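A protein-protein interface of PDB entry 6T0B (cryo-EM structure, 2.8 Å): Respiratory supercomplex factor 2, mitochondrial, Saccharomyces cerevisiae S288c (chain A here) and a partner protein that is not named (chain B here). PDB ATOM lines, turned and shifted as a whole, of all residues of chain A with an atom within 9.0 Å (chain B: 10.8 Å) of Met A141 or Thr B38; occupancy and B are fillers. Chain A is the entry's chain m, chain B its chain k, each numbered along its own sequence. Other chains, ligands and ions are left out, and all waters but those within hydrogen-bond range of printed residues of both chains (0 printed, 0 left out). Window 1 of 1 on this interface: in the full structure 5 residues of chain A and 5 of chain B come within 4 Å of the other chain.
OE1 of Gln A149 lies within hydrogen-bond range of NE1 of Trp B42 (3.3 Å).
OG1 of Thr B31 lies within hydrogen-bond range of O of Ser B27.
The side-chain hydroxyl (OG1) of Thr B38 sits at hydrogen-bond distance from the backbone carbonyl oxygen (O) of His B34 (2.6 Å).
The side-chain hydroxyl (OG) of Ser B46 sits close to the backbone carbonyl oxygen (O) of Trp B42 (3.3 Å).
NE2 of Gln A149 lies within hydrogen-bond range of SD of Met A141 (3.0 Å).
O of Gln A145 sits at hydrogen-bond distance from NE2 of Gln A149, 3.2 Å away.
Among the printed residues, pairs that only touch across the chains: Ile A140 with His B34, Met A141 with His B34, Tyr A153 with Trp B42, Ile A140 with Ala B30, Ile A140 with Thr B31 and Met A141 with Thr B38.
Met A141 touches two residues of chain B.
Thr B38 touches one residue of chain A.
No residue of chain B comes within 4 Å of Thr A142.
No residue of chain B comes within 4 Å of Gln A145.
No residue of chain A comes within 4 Å of Ser B39.
Printed residues of chain B within 4 Å of Gln A149: Trp B42.
Printed residues of chain A within 4 Å of Thr B31: Ile A140.
Pro A139 touches none of the printed residues of chain B.
Val A148 touches none of the printed residues of chain B.
The nearest printed residue of chain B that does not touch Met A141 is Trp B42 (5.7 Å).
The nearest printed residue of chain B that does not touch Tyr A153 is Ile B45 (4.1 Å).
Along chain B the printed residues that touch a printed residue of chain A span positions 30 to 42.
Hydrophobic or aromatic side chains of chain A within 4 Å of the printed part of chain B: Ile A140, Met A141 and Tyr A153.
Along chain A the printed residues that touch a printed residue of chain B span positions 140 to 153.
Among the printed residues, 7 pairs touch across the chains.
Among the printed residues, no Asp or Glu carboxylate lies within 4 Å of a Lys or Arg side-chain nitrogen of the other chain.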
ATOM      1  N   TRP A 132      10.346 -28.378 -14.134  1.00  0.00           N
ATOM      2  CA  TRP A 132      11.519 -28.894 -14.822  1.00  0.00           C
ATOM      3  C   TRP A 132      12.375 -27.780 -15.407  1.00  0.00           C
ATOM      4  O   TRP A 132      13.604 -27.832 -15.315  1.00  0.00           O
ATOM      5  CB  TRP A 132      11.090 -29.862 -15.921  1.00  0.00           C
ATOM      6  CG  TRP A 132      12.222 -30.302 -16.770  1.00  0.00           C
ATOM      7  CD1 TRP A 132      12.428 -29.995 -18.081  1.00  0.00           C
ATOM      8  CD2 TRP A 132      13.321 -31.127 -16.371  1.00  0.00           C
ATOM      9  NE1 TRP A 132      13.588 -30.582 -18.526  1.00  0.00           N
ATOM     10  CE2 TRP A 132      14.154 -31.282 -17.493  1.00  0.00           C
ATOM     11  CE3 TRP A 132      13.679 -31.750 -15.174  1.00  0.00           C
ATOM     12  CZ2 TRP A 132      15.320 -32.034 -17.454  1.00  0.00           C
ATOM     13  CZ3 TRP A 132      14.836 -32.487 -15.135  1.00  0.00           C
ATOM     14  CH2 TRP A 132      15.643 -32.629 -16.268  1.00  0.00           C
ATOM     15  N   ILE A 134      12.479 -24.630 -14.362  1.00  0.00           N
ATOM     16  CA  ILE A 134      13.034 -23.830 -13.273  1.00  0.00           C
ATOM     17  C   ILE A 134      14.156 -24.593 -12.560  1.00  0.00           C
ATOM     18  O   ILE A 134      15.140 -23.991 -12.115  1.00  0.00           O
ATOM     19  CB  ILE A 134      11.903 -23.364 -12.319  1.00  0.00           C
ATOM     20  CG1 ILE A 134      10.990 -22.341 -13.014  1.00  0.00           C
ATOM     21  CG2 ILE A 134      12.427 -22.750 -11.013  1.00  0.00           C
ATOM     22  CD1 ILE A 134       9.721 -22.880 -13.592  1.00  0.00           C
ATOM     23  N   VAL A 135      14.088 -25.922 -12.507  1.00  0.00           N
ATOM     24  CA  VAL A 135      15.200 -26.656 -11.909  1.00  0.00           C
ATOM     25  C   VAL A 135      16.336 -26.882 -12.912  1.00  0.00           C
ATOM     26  O   VAL A 135      17.490 -27.055 -12.507  1.00  0.00           O
ATOM     27  CB  VAL A 135      14.712 -27.982 -11.284  1.00  0.00           C
ATOM     28  CG1 VAL A 135      14.418 -29.036 -12.342  1.00  0.00           C
ATOM     29  CG2 VAL A 135      15.705 -28.505 -10.232  1.00  0.00           C
ATOM     30  N   ASN A 136      16.054 -26.831 -14.214  1.00  0.00           N
ATOM     31  CA  ASN A 136      17.064 -27.075 -15.233  1.00  0.00           C
ATOM     32  C   ASN A 136      17.743 -25.802 -15.728  1.00  0.00           C
ATOM     33  O   ASN A 136      18.755 -25.893 -16.430  1.00  0.00           O
ATOM     34  CB  ASN A 136      16.430 -27.818 -16.415  1.00  0.00           C
ATOM     35  CG  ASN A 136      17.443 -28.568 -17.248  1.00  0.00           C
ATOM     36  OD1 ASN A 136      18.581 -28.766 -16.831  1.00  0.00           O
ATOM     37  ND2 ASN A 136      17.034 -28.991 -18.436  1.00  0.00           N
ATOM     38  N   ASP A 138      19.471 -23.698 -14.033  1.00  0.00           N
ATOM     39  CA  ASP A 138      20.747 -23.503 -13.346  1.00  0.00           C
ATOM     40  C   ASP A 138      21.518 -24.816 -13.324  1.00  0.00           C
ATOM     41  O   ASP A 138      21.511 -25.530 -12.311  1.00  0.00           O
ATOM     42  CB  ASP A 138      20.532 -22.976 -11.927  1.00  0.00           C
ATOM     43  CG  ASP A 138      20.464 -21.467 -11.877  1.00  0.00           C
ATOM     44  OD1 ASP A 138      19.801 -20.930 -10.967  1.00  0.00           O
ATOM     45  OD2 ASP A 138      21.061 -20.814 -12.758  1.00  0.00           O
ATOM     46  N   PRO A 139      22.206 -25.179 -14.409  1.00  0.00           N
ATOM     47  CA  PRO A 139      22.799 -26.517 -14.492  1.00  0.00           C
ATOM     48  C   PRO A 139      24.189 -26.645 -13.897  1.00  0.00           C
ATOM     49  O   PRO A 139      25.161 -26.097 -14.425  1.00  0.00           O
ATOM     50  CB  PRO A 139      22.829 -26.781 -16.003  1.00  0.00           C
ATOM     51  CG  PRO A 139      22.788 -25.405 -16.655  1.00  0.00           C
ATOM     52  CD  PRO A 139      22.528 -24.370 -15.595  1.00  0.00           C
ATOM     53  N   ILE A 140      24.291 -27.353 -12.776  1.00  0.00           N
ATOM     54  CA  ILE A 140      25.513 -28.074 -12.435  1.00  0.00           C
ATOM     55  C   ILE A 140      25.234 -29.493 -11.957  1.00  0.00           C
ATOM     56  O   ILE A 140      26.106 -30.374 -12.080  1.00  0.00           O
ATOM     57  CB  ILE A 140      26.333 -27.278 -11.388  1.00  0.00           C
ATOM     58  CG1 ILE A 140      27.754 -27.828 -11.193  1.00  0.00           C
ATOM     59  CG2 ILE A 140      25.602 -27.205 -10.101  1.00  0.00           C
ATOM     60  CD1 ILE A 140      28.661 -26.907 -10.421  1.00  0.00           C
ATOM     61  N   MET A 141      24.018 -29.798 -11.500  1.00  0.00           N
ATOM     62  CA  MET A 141      23.661 -31.159 -11.136  1.00  0.00           C
ATOM     63  C   MET A 141      23.512 -32.023 -12.379  1.00  0.00           C
ATOM     64  O   MET A 141      23.267 -31.531 -13.482  1.00  0.00           O
ATOM     65  CB  MET A 141      22.347 -31.199 -10.360  1.00  0.00           C
ATOM     66  CG  MET A 141      22.118 -30.097  -9.345  1.00  0.00           C
ATOM     67  SD  MET A 141      20.927 -30.667  -8.113  1.00  0.00           S
ATOM     68  CE  MET A 141      20.443 -29.137  -7.331  1.00  0.00           C
ATOM     69  N   THR A 142      23.659 -33.327 -12.181  1.00  0.00           N
ATOM     70  CA  THR A 142      23.338 -34.304 -13.206  1.00  0.00           C
ATOM     71  C   THR A 142      21.814 -34.356 -13.368  1.00  0.00           C
ATOM     72  O   THR A 142      21.068 -33.938 -12.478  1.00  0.00           O
ATOM     73  CB  THR A 142      23.969 -35.650 -12.813  1.00  0.00           C
ATOM     74  OG1 THR A 142      25.362 -35.438 -12.555  1.00  0.00           O
ATOM     75  CG2 THR A 142      23.883 -36.718 -13.908  1.00  0.00           C
ATOM     76  N   LYS A 143      21.361 -34.828 -14.543  1.00  0.00           N
ATOM     77  CA  LYS A 143      19.949 -34.799 -14.926  1.00  0.00           C
ATOM     78  C   LYS A 143      19.056 -35.568 -13.957  1.00  0.00           C
ATOM     79  O   LYS A 143      17.903 -35.176 -13.747  1.00  0.00           O
ATOM     80  CB  LYS A 143      19.784 -35.370 -16.334  1.00  0.00           C
ATOM     81  CG  LYS A 143      20.604 -34.673 -17.405  1.00  0.00           C
ATOM     82  CD  LYS A 143      21.092 -35.649 -18.468  1.00  0.00           C
ATOM     83  CE  LYS A 143      22.396 -36.325 -18.061  1.00  0.00           C
ATOM     84  NZ  LYS A 143      22.874 -37.308 -19.079  1.00  0.00           N
ATOM     85  N   ALA A 144      19.578 -36.633 -13.338  1.00  0.00           N
ATOM     86  CA  ALA A 144      18.778 -37.428 -12.410  1.00  0.00           C
ATOM     87  C   ALA A 144      18.427 -36.644 -11.151  1.00  0.00           C
ATOM     88  O   ALA A 144      17.299 -36.741 -10.651  1.00  0.00           O
ATOM     89  CB  ALA A 144      19.516 -38.714 -12.049  1.00  0.00           C
ATOM     90  N   GLN A 145      19.371 -35.850 -10.632  1.00  0.00           N
ATOM     91  CA  GLN A 145      19.088 -35.044  -9.448  1.00  0.00           C
ATOM     92  C   GLN A 145      18.087 -33.934  -9.752  1.00  0.00           C
ATOM     93  O   GLN A 145      17.230 -33.623  -8.910  1.00  0.00           O
ATOM     94  CB  GLN A 145      20.387 -34.479  -8.874  1.00  0.00           C
ATOM     95  CG  GLN A 145      21.424 -35.547  -8.572  1.00  0.00           C
ATOM     96  CD  GLN A 145      22.848 -35.020  -8.581  1.00  0.00           C
ATOM     97  OE1 GLN A 145      23.080 -33.825  -8.420  1.00  0.00           O
ATOM     98  NE2 GLN A 145      23.809 -35.916  -8.767  1.00  0.00           N
ATOM     99  N   LYS A 146      18.149 -33.367 -10.960  1.00  0.00           N
ATOM    100  CA  LYS A 146      17.140 -32.401 -11.386  1.00  0.00           C
ATOM    101  C   LYS A 146      15.761 -33.039 -11.479  1.00  0.00           C
ATOM    102  O   LYS A 146      14.767 -32.431 -11.058  1.00  0.00           O
ATOM    103  CB  LYS A 146      17.524 -31.790 -12.730  1.00  0.00           C
ATOM    104  CG  LYS A 146      18.780 -30.944 -12.704  1.00  0.00           C
ATOM    105  CD  LYS A 146      19.178 -30.527 -14.102  1.00  0.00           C
ATOM    106  CE  LYS A 146      20.465 -29.739 -14.098  1.00  0.00           C
ATOM    107  NZ  LYS A 146      20.950 -29.532 -15.485  1.00  0.00           N
ATOM    108  N   ILE A 147      15.686 -34.267 -12.016  1.00  0.00           N
ATOM    109  CA  ILE A 147      14.404 -34.969 -12.120  1.00  0.00           C
ATOM    110  C   ILE A 147      13.830 -35.250 -10.737  1.00  0.00           C
ATOM    111  O   ILE A 147      12.641 -35.010 -10.487  1.00  0.00           O
ATOM    112  CB  ILE A 147      14.548 -36.266 -12.942  1.00  0.00           C
ATOM    113  CG1 ILE A 147      14.873 -35.961 -14.398  1.00  0.00           C
ATOM    114  CG2 ILE A 147      13.263 -37.070 -12.919  1.00  0.00           C
ATOM    115  CD1 ILE A 147      15.315 -37.167 -15.190  1.00  0.00           C
ATOM    116  N   VAL A 148      14.673 -35.707  -9.804  1.00  0.00           N
ATOM    117  CA  VAL A 148      14.135 -36.094  -8.504  1.00  0.00           C
ATOM    118  C   VAL A 148      13.750 -34.865  -7.686  1.00  0.00           C
ATOM    119  O   VAL A 148      12.763 -34.903  -6.945  1.00  0.00           O
ATOM    120  CB  VAL A 148      15.102 -37.027  -7.736  1.00  0.00           C
ATOM    121  CG1 VAL A 148      15.360 -38.310  -8.530  1.00  0.00           C
ATOM    122  CG2 VAL A 148      16.395 -36.344  -7.305  1.00  0.00           C
ATOM    123  N   GLN A 149      14.431 -33.731  -7.872  1.00  0.00           N
ATOM    124  CA  GLN A 149      14.021 -32.550  -7.117  1.00  0.00           C
ATOM    125  C   GLN A 149      12.781 -31.880  -7.713  1.00  0.00           C
ATOM    126  O   GLN A 149      11.909 -31.411  -6.962  1.00  0.00           O
ATOM    127  CB  GLN A 149      15.182 -31.568  -7.013  1.00  0.00           C
ATOM    128  CG  GLN A 149      16.281 -32.075  -6.123  1.00  0.00           C
ATOM    129  CD  GLN A 149      17.529 -31.248  -6.220  1.00  0.00           C
ATOM    130  OE1 GLN A 149      17.514 -30.047  -5.963  1.00  0.00           O
ATOM    131  NE2 GLN A 149      18.625 -31.884  -6.601  1.00  0.00           N
ATOM    132  N   ALA A 150      12.671 -31.839  -9.050  1.00  0.00           N
ATOM    133  CA  ALA A 150      11.464 -31.311  -9.678  1.00  0.00           C
ATOM    134  C   ALA A 150      10.251 -32.167  -9.338  1.00  0.00           C
ATOM    135  O   ALA A 150       9.171 -31.640  -9.042  1.00  0.00           O
ATOM    136  CB  ALA A 150      11.654 -31.232 -11.191  1.00  0.00           C
ATOM    137  N   TYR A 153       9.202 -31.521  -5.627  1.00  0.00           N
ATOM    138  CA  TYR A 153       8.332 -30.356  -5.497  1.00  0.00           C
ATOM    139  C   TYR A 153       6.934 -30.655  -6.030  1.00  0.00           C
ATOM    140  O   TYR A 153       5.925 -30.315  -5.383  1.00  0.00           O
ATOM    141  CB  TYR A 153       8.940 -29.158  -6.225  1.00  0.00           C
ATOM    142  CG  TYR A 153      10.284 -28.714  -5.703  1.00  0.00           C
ATOM    143  CD1 TYR A 153      10.553 -28.706  -4.340  1.00  0.00           C
ATOM    144  CD2 TYR A 153      11.280 -28.294  -6.574  1.00  0.00           C
ATOM    145  CE1 TYR A 153      11.782 -28.293  -3.857  1.00  0.00           C
ATOM    146  CE2 TYR A 153      12.514 -27.879  -6.101  1.00  0.00           C
ATOM    147  CZ  TYR A 153      12.756 -27.882  -4.743  1.00  0.00           C
ATOM    148  OH  TYR A 153      13.979 -27.469  -4.273  1.00  0.00           O
ATOM    149  N   SER B  27      35.132 -28.779 -12.043  1.00  0.00           N
ATOM    150  CA  SER B  27      33.844 -29.410 -11.774  1.00  0.00           C
ATOM    151  C   SER B  27      33.926 -30.285 -10.531  1.00  0.00           C
ATOM    152  O   SER B  27      32.977 -30.334  -9.732  1.00  0.00           O
ATOM    153  CB  SER B  27      33.389 -30.211 -12.988  1.00  0.00           C
ATOM    154  OG  SER B  27      33.556 -29.450 -14.168  1.00  0.00           O
ATOM    155  N   ALA B  30      33.594 -27.755  -7.833  1.00  0.00           N
ATOM    156  CA  ALA B  30      32.391 -26.930  -7.884  1.00  0.00           C
ATOM    157  C   ALA B  30      31.123 -27.698  -7.558  1.00  0.00           C
ATOM    158  O   ALA B  30      30.183 -27.120  -6.996  1.00  0.00           O
ATOM    159  CB  ALA B  30      32.235 -26.290  -9.266  1.00  0.00           C
ATOM    160  N   THR B  31      31.071 -28.994  -7.868  1.00  0.00           N
ATOM    161  CA  THR B  31      29.959 -29.775  -7.349  1.00  0.00           C
ATOM    162  C   THR B  31      30.053 -29.958  -5.838  1.00  0.00           C
ATOM    163  O   THR B  31      29.020 -30.162  -5.203  1.00  0.00           O
ATOM    164  CB  THR B  31      29.855 -31.123  -8.062  1.00  0.00           C
ATOM    165  OG1 THR B  31      31.154 -31.702  -8.201  1.00  0.00           O
ATOM    166  CG2 THR B  31      29.230 -30.945  -9.442  1.00  0.00           C
ATOM    167  N   GLU B  32      31.244 -29.793  -5.244  1.00  0.00           N
ATOM    168  CA  GLU B  32      31.363 -29.743  -3.788  1.00  0.00           C
ATOM    169  C   GLU B  32      30.644 -28.526  -3.209  1.00  0.00           C
ATOM    170  O   GLU B  32      29.859 -28.658  -2.258  1.00  0.00           O
ATOM    171  CB  GLU B  32      32.841 -29.739  -3.376  1.00  0.00           C
ATOM    172  CG  GLU B  32      33.126 -30.203  -1.936  1.00  0.00           C
ATOM    173  CD  GLU B  32      32.890 -29.131  -0.869  1.00  0.00           C
ATOM    174  OE1 GLU B  32      32.684 -29.493   0.310  1.00  0.00           O
ATOM    175  OE2 GLU B  32      32.927 -27.928  -1.200  1.00  0.00           O
ATOM    176  N   LYS B  33      30.924 -27.327  -3.744  1.00  0.00           N
ATOM    177  CA  LYS B  33      30.321 -26.117  -3.187  1.00  0.00           C
ATOM    178  C   LYS B  33      28.818 -26.090  -3.446  1.00  0.00           C
ATOM    179  O   LYS B  33      28.027 -25.730  -2.553  1.00  0.00           O
ATOM    180  CB  LYS B  33      31.020 -24.856  -3.732  1.00  0.00           C
ATOM    181  CG  LYS B  33      30.909 -24.576  -5.234  1.00  0.00           C
ATOM    182  CD  LYS B  33      31.651 -23.329  -5.698  1.00  0.00           C
ATOM    183  CE  LYS B  33      30.941 -22.062  -5.254  1.00  0.00           C
ATOM    184  NZ  LYS B  33      29.603 -21.919  -5.895  1.00  0.00           N
ATOM    185  N   HIS B  34      28.397 -26.565  -4.621  1.00  0.00           N
ATOM    186  CA  HIS B  34      26.972 -26.596  -4.895  1.00  0.00           C
ATOM    187  C   HIS B  34      26.271 -27.698  -4.114  1.00  0.00           C
ATOM    188  O   HIS B  34      25.102 -27.543  -3.755  1.00  0.00           O
ATOM    189  CB  HIS B  34      26.724 -26.762  -6.379  1.00  0.00           C
ATOM    190  CG  HIS B  34      25.302 -26.544  -6.761  1.00  0.00           C
ATOM    191  ND1 HIS B  34      24.422 -27.584  -6.956  1.00  0.00           N
ATOM    192  CD2 HIS B  34      24.605 -25.409  -6.986  1.00  0.00           C
ATOM    193  CE1 HIS B  34      23.242 -27.095  -7.292  1.00  0.00           C
ATOM    194  NE2 HIS B  34      23.324 -25.779  -7.312  1.00  0.00           N
ATOM    195  N   ALA B  35      26.977 -28.786  -3.792  1.00  0.00           N
ATOM    196  CA  ALA B  35      26.396 -29.824  -2.958  1.00  0.00           C
ATOM    197  C   ALA B  35      26.268 -29.374  -1.515  1.00  0.00           C
ATOM    198  O   ALA B  35      25.321 -29.777  -0.831  1.00  0.00           O
ATOM    199  CB  ALA B  35      27.241 -31.092  -3.047  1.00  0.00           C
ATOM    200  N   LYS B  36      27.196 -28.536  -1.038  1.00  0.00           N
ATOM    201  CA  LYS B  36      27.057 -27.984   0.307  1.00  0.00           C
ATOM    202  C   LYS B  36      25.858 -27.051   0.399  1.00  0.00           C
ATOM    203  O   LYS B  36      25.073 -27.133   1.356  1.00  0.00           O
ATOM    204  CB  LYS B  36      28.337 -27.263   0.724  1.00  0.00           C
ATOM    205  CG  LYS B  36      28.425 -26.994   2.214  1.00  0.00           C
ATOM    206  CD  LYS B  36      29.531 -26.007   2.544  1.00  0.00           C
ATOM    207  CE  LYS B  36      28.970 -24.622   2.834  1.00  0.00           C
ATOM    208  NZ  LYS B  36      28.098 -24.598   4.046  1.00  0.00           N
ATOM    209  N   ASP B  37      25.676 -26.185  -0.604  1.00  0.00           N
ATOM    210  CA  ASP B  37      24.513 -25.298  -0.584  1.00  0.00           C
ATOM    211  C   ASP B  37      23.205 -26.071  -0.771  1.00  0.00           C
ATOM    212  O   ASP B  37      22.178 -25.742  -0.159  1.00  0.00           O
ATOM    213  CB  ASP B  37      24.653 -24.213  -1.648  1.00  0.00           C
ATOM    214  CG  ASP B  37      23.582 -23.148  -1.520  1.00  0.00           C
ATOM    215  OD1 ASP B  37      23.153 -22.597  -2.556  1.00  0.00           O
ATOM    216  OD2 ASP B  37      23.157 -22.877  -0.376  1.00  0.00           O
ATOM    217  N   THR B  38      23.238 -27.121  -1.601  1.00  0.00           N
ATOM    218  CA  THR B  38      22.071 -27.965  -1.823  1.00  0.00           C
ATOM    219  C   THR B  38      21.687 -28.719  -0.556  1.00  0.00           C
ATOM    220  O   THR B  38      20.499 -28.826  -0.225  1.00  0.00           O
ATOM    221  CB  THR B  38      22.367 -28.932  -2.968  1.00  0.00           C
ATOM    222  OG1 THR B  38      22.625 -28.186  -4.162  1.00  0.00           O
ATOM    223  CG2 THR B  38      21.208 -29.847  -3.227  1.00  0.00           C
ATOM    224  N   SER B  39      22.686 -29.201   0.190  1.00  0.00           N
ATOM    225  CA  SER B  39      22.417 -29.868   1.455  1.00  0.00           C
ATOM    226  C   SER B  39      21.845 -28.898   2.472  1.00  0.00           C
ATOM    227  O   SER B  39      20.957 -29.264   3.255  1.00  0.00           O
ATOM    228  CB  SER B  39      23.712 -30.466   1.995  1.00  0.00           C
ATOM    229  OG  SER B  39      24.313 -31.261   1.010  1.00  0.00           O
ATOM    230  N   ASN B  40      22.344 -27.657   2.463  1.00  0.00           N
ATOM    231  CA  ASN B  40      21.863 -26.633   3.384  1.00  0.00           C
ATOM    232  C   ASN B  40      20.390 -26.340   3.152  1.00  0.00           C
ATOM    233  O   ASN B  40      19.572 -26.412   4.081  1.00  0.00           O
ATOM    234  CB  ASN B  40      22.703 -25.365   3.219  1.00  0.00           C
ATOM    235  CG  ASN B  40      22.255 -24.239   4.134  1.00  0.00           C
ATOM    236  OD1 ASN B  40      22.584 -24.224   5.319  1.00  0.00           O
ATOM    237  ND2 ASN B  40      21.516 -23.278   3.583  1.00  0.00           N
ATOM    238  N   MET B  41      20.024 -26.059   1.899  1.00  0.00           N
ATOM    239  CA  MET B  41      18.625 -25.766   1.610  1.00  0.00           C
ATOM    240  C   MET B  41      17.733 -26.999   1.720  1.00  0.00           C
ATOM    241  O   MET B  41      16.542 -26.856   2.009  1.00  0.00           O
ATOM    242  CB  MET B  41      18.483 -25.129   0.233  1.00  0.00           C
ATOM    243  CG  MET B  41      18.851 -26.017  -0.924  1.00  0.00           C
ATOM    244  SD  MET B  41      18.280 -25.288  -2.465  1.00  0.00           S
ATOM    245  CE  MET B  41      16.559 -25.014  -2.057  1.00  0.00           C
ATOM    246  N   TRP B  42      18.278 -28.209   1.588  1.00  0.00           N
ATOM    247  CA  TRP B  42      17.400 -29.365   1.708  1.00  0.00           C
ATOM    248  C   TRP B  42      17.166 -29.782   3.153  1.00  0.00           C
ATOM    249  O   TRP B  42      16.086 -30.289   3.464  1.00  0.00           O
ATOM    250  CB  TRP B  42      17.939 -30.536   0.895  1.00  0.00           C
ATOM    251  CG  TRP B  42      17.417 -30.546  -0.501  1.00  0.00           C
ATOM    252  CD1 TRP B  42      18.132 -30.349  -1.636  1.00  0.00           C
ATOM    253  CD2 TRP B  42      16.064 -30.750  -0.912  1.00  0.00           C
ATOM    254  NE1 TRP B  42      17.316 -30.423  -2.734  1.00  0.00           N
ATOM    255  CE2 TRP B  42      16.038 -30.671  -2.312  1.00  0.00           C
ATOM    256  CE3 TRP B  42      14.875 -31.005  -0.233  1.00  0.00           C
ATOM    257  CZ2 TRP B  42      14.872 -30.826  -3.041  1.00  0.00           C
ATOM    258  CZ3 TRP B  42      13.724 -31.161  -0.960  1.00  0.00           C
ATOM    259  CH2 TRP B  42      13.730 -31.076  -2.347  1.00  0.00           C
ATOM    260  N   VAL B  43      18.133 -29.574   4.054  1.00  0.00           N
ATOM    261  CA  VAL B  43      17.829 -29.741   5.476  1.00  0.00           C
ATOM    262  C   VAL B  43      16.876 -28.639   5.934  1.00  0.00           C
ATOM    263  O   VAL B  43      15.983 -28.883   6.766  1.00  0.00           O
ATOM    264  CB  VAL B  43      19.126 -29.780   6.313  1.00  0.00           C
ATOM    265  CG1 VAL B  43      18.843 -29.808   7.816  1.00  0.00           C
ATOM    266  CG2 VAL B  43      19.981 -30.951   5.918  1.00  0.00           C
ATOM    267  N   LYS B  44      17.017 -27.434   5.361  1.00  0.00           N
ATOM    268  CA  LYS B  44      16.062 -26.358   5.616  1.00  0.00           C
ATOM    269  C   LYS B  44      14.647 -26.762   5.213  1.00  0.00           C
ATOM    270  O   LYS B  44      13.698 -26.574   5.983  1.00  0.00           O
ATOM    271  CB  LYS B  44      16.494 -25.095   4.873  1.00  0.00           C
ATOM    272  CG  LYS B  44      16.151 -23.809   5.593  1.00  0.00           C
ATOM    273  CD  LYS B  44      16.275 -22.605   4.684  1.00  0.00           C
ATOM    274  CE  LYS B  44      15.787 -21.345   5.383  1.00  0.00           C
ATOM    275  NZ  LYS B  44      15.581 -20.214   4.435  1.00  0.00           N
ATOM    276  N   ILE B  45      14.502 -27.386   4.043  1.00  0.00           N
ATOM    277  CA  ILE B  45      13.185 -27.849   3.607  1.00  0.00           C
ATOM    278  C   ILE B  45      12.699 -29.013   4.471  1.00  0.00           C
ATOM    279  O   ILE B  45      11.542 -29.029   4.915  1.00  0.00           O
ATOM    280  CB  ILE B  45      13.222 -28.209   2.109  1.00  0.00           C
ATOM    281  CG1 ILE B  45      13.294 -26.936   1.262  1.00  0.00           C
ATOM    282  CG2 ILE B  45      12.006 -29.026   1.698  1.00  0.00           C
ATOM    283  CD1 ILE B  45      13.360 -27.189  -0.219  1.00  0.00           C
ATOM    284  N   SER B  46      13.585 -29.967   4.782  1.00  0.00           N
ATOM    285  CA  SER B  46      13.221 -31.172   5.519  1.00  0.00           C
ATOM    286  C   SER B  46      12.870 -30.911   6.973  1.00  0.00           C
ATOM    287  O   SER B  46      12.281 -31.789   7.608  1.00  0.00           O
ATOM    288  CB  SER B  46      14.354 -32.195   5.495  1.00  0.00           C
ATOM    289  OG  SER B  46      15.398 -31.817   6.362  1.00  0.00           O
ATOM    290  N   VAL B  47      13.264 -29.773   7.539  1.00  0.00           N
ATOM    291  CA  VAL B  47      12.853 -29.438   8.889  1.00  0.00           C
ATOM    292  C   VAL B  47      11.794 -28.335   8.926  1.00  0.00           C
ATOM    293  O   VAL B  47      11.048 -28.248   9.908  1.00  0.00           O
ATOM    294  CB  VAL B  47      14.069 -29.076   9.773  1.00  0.00           C
ATOM    295  CG1 VAL B  47      14.516 -27.645   9.559  1.00  0.00           C
ATOM    296  CG2 VAL B  47      13.788 -29.357  11.241  1.00  0.00           C
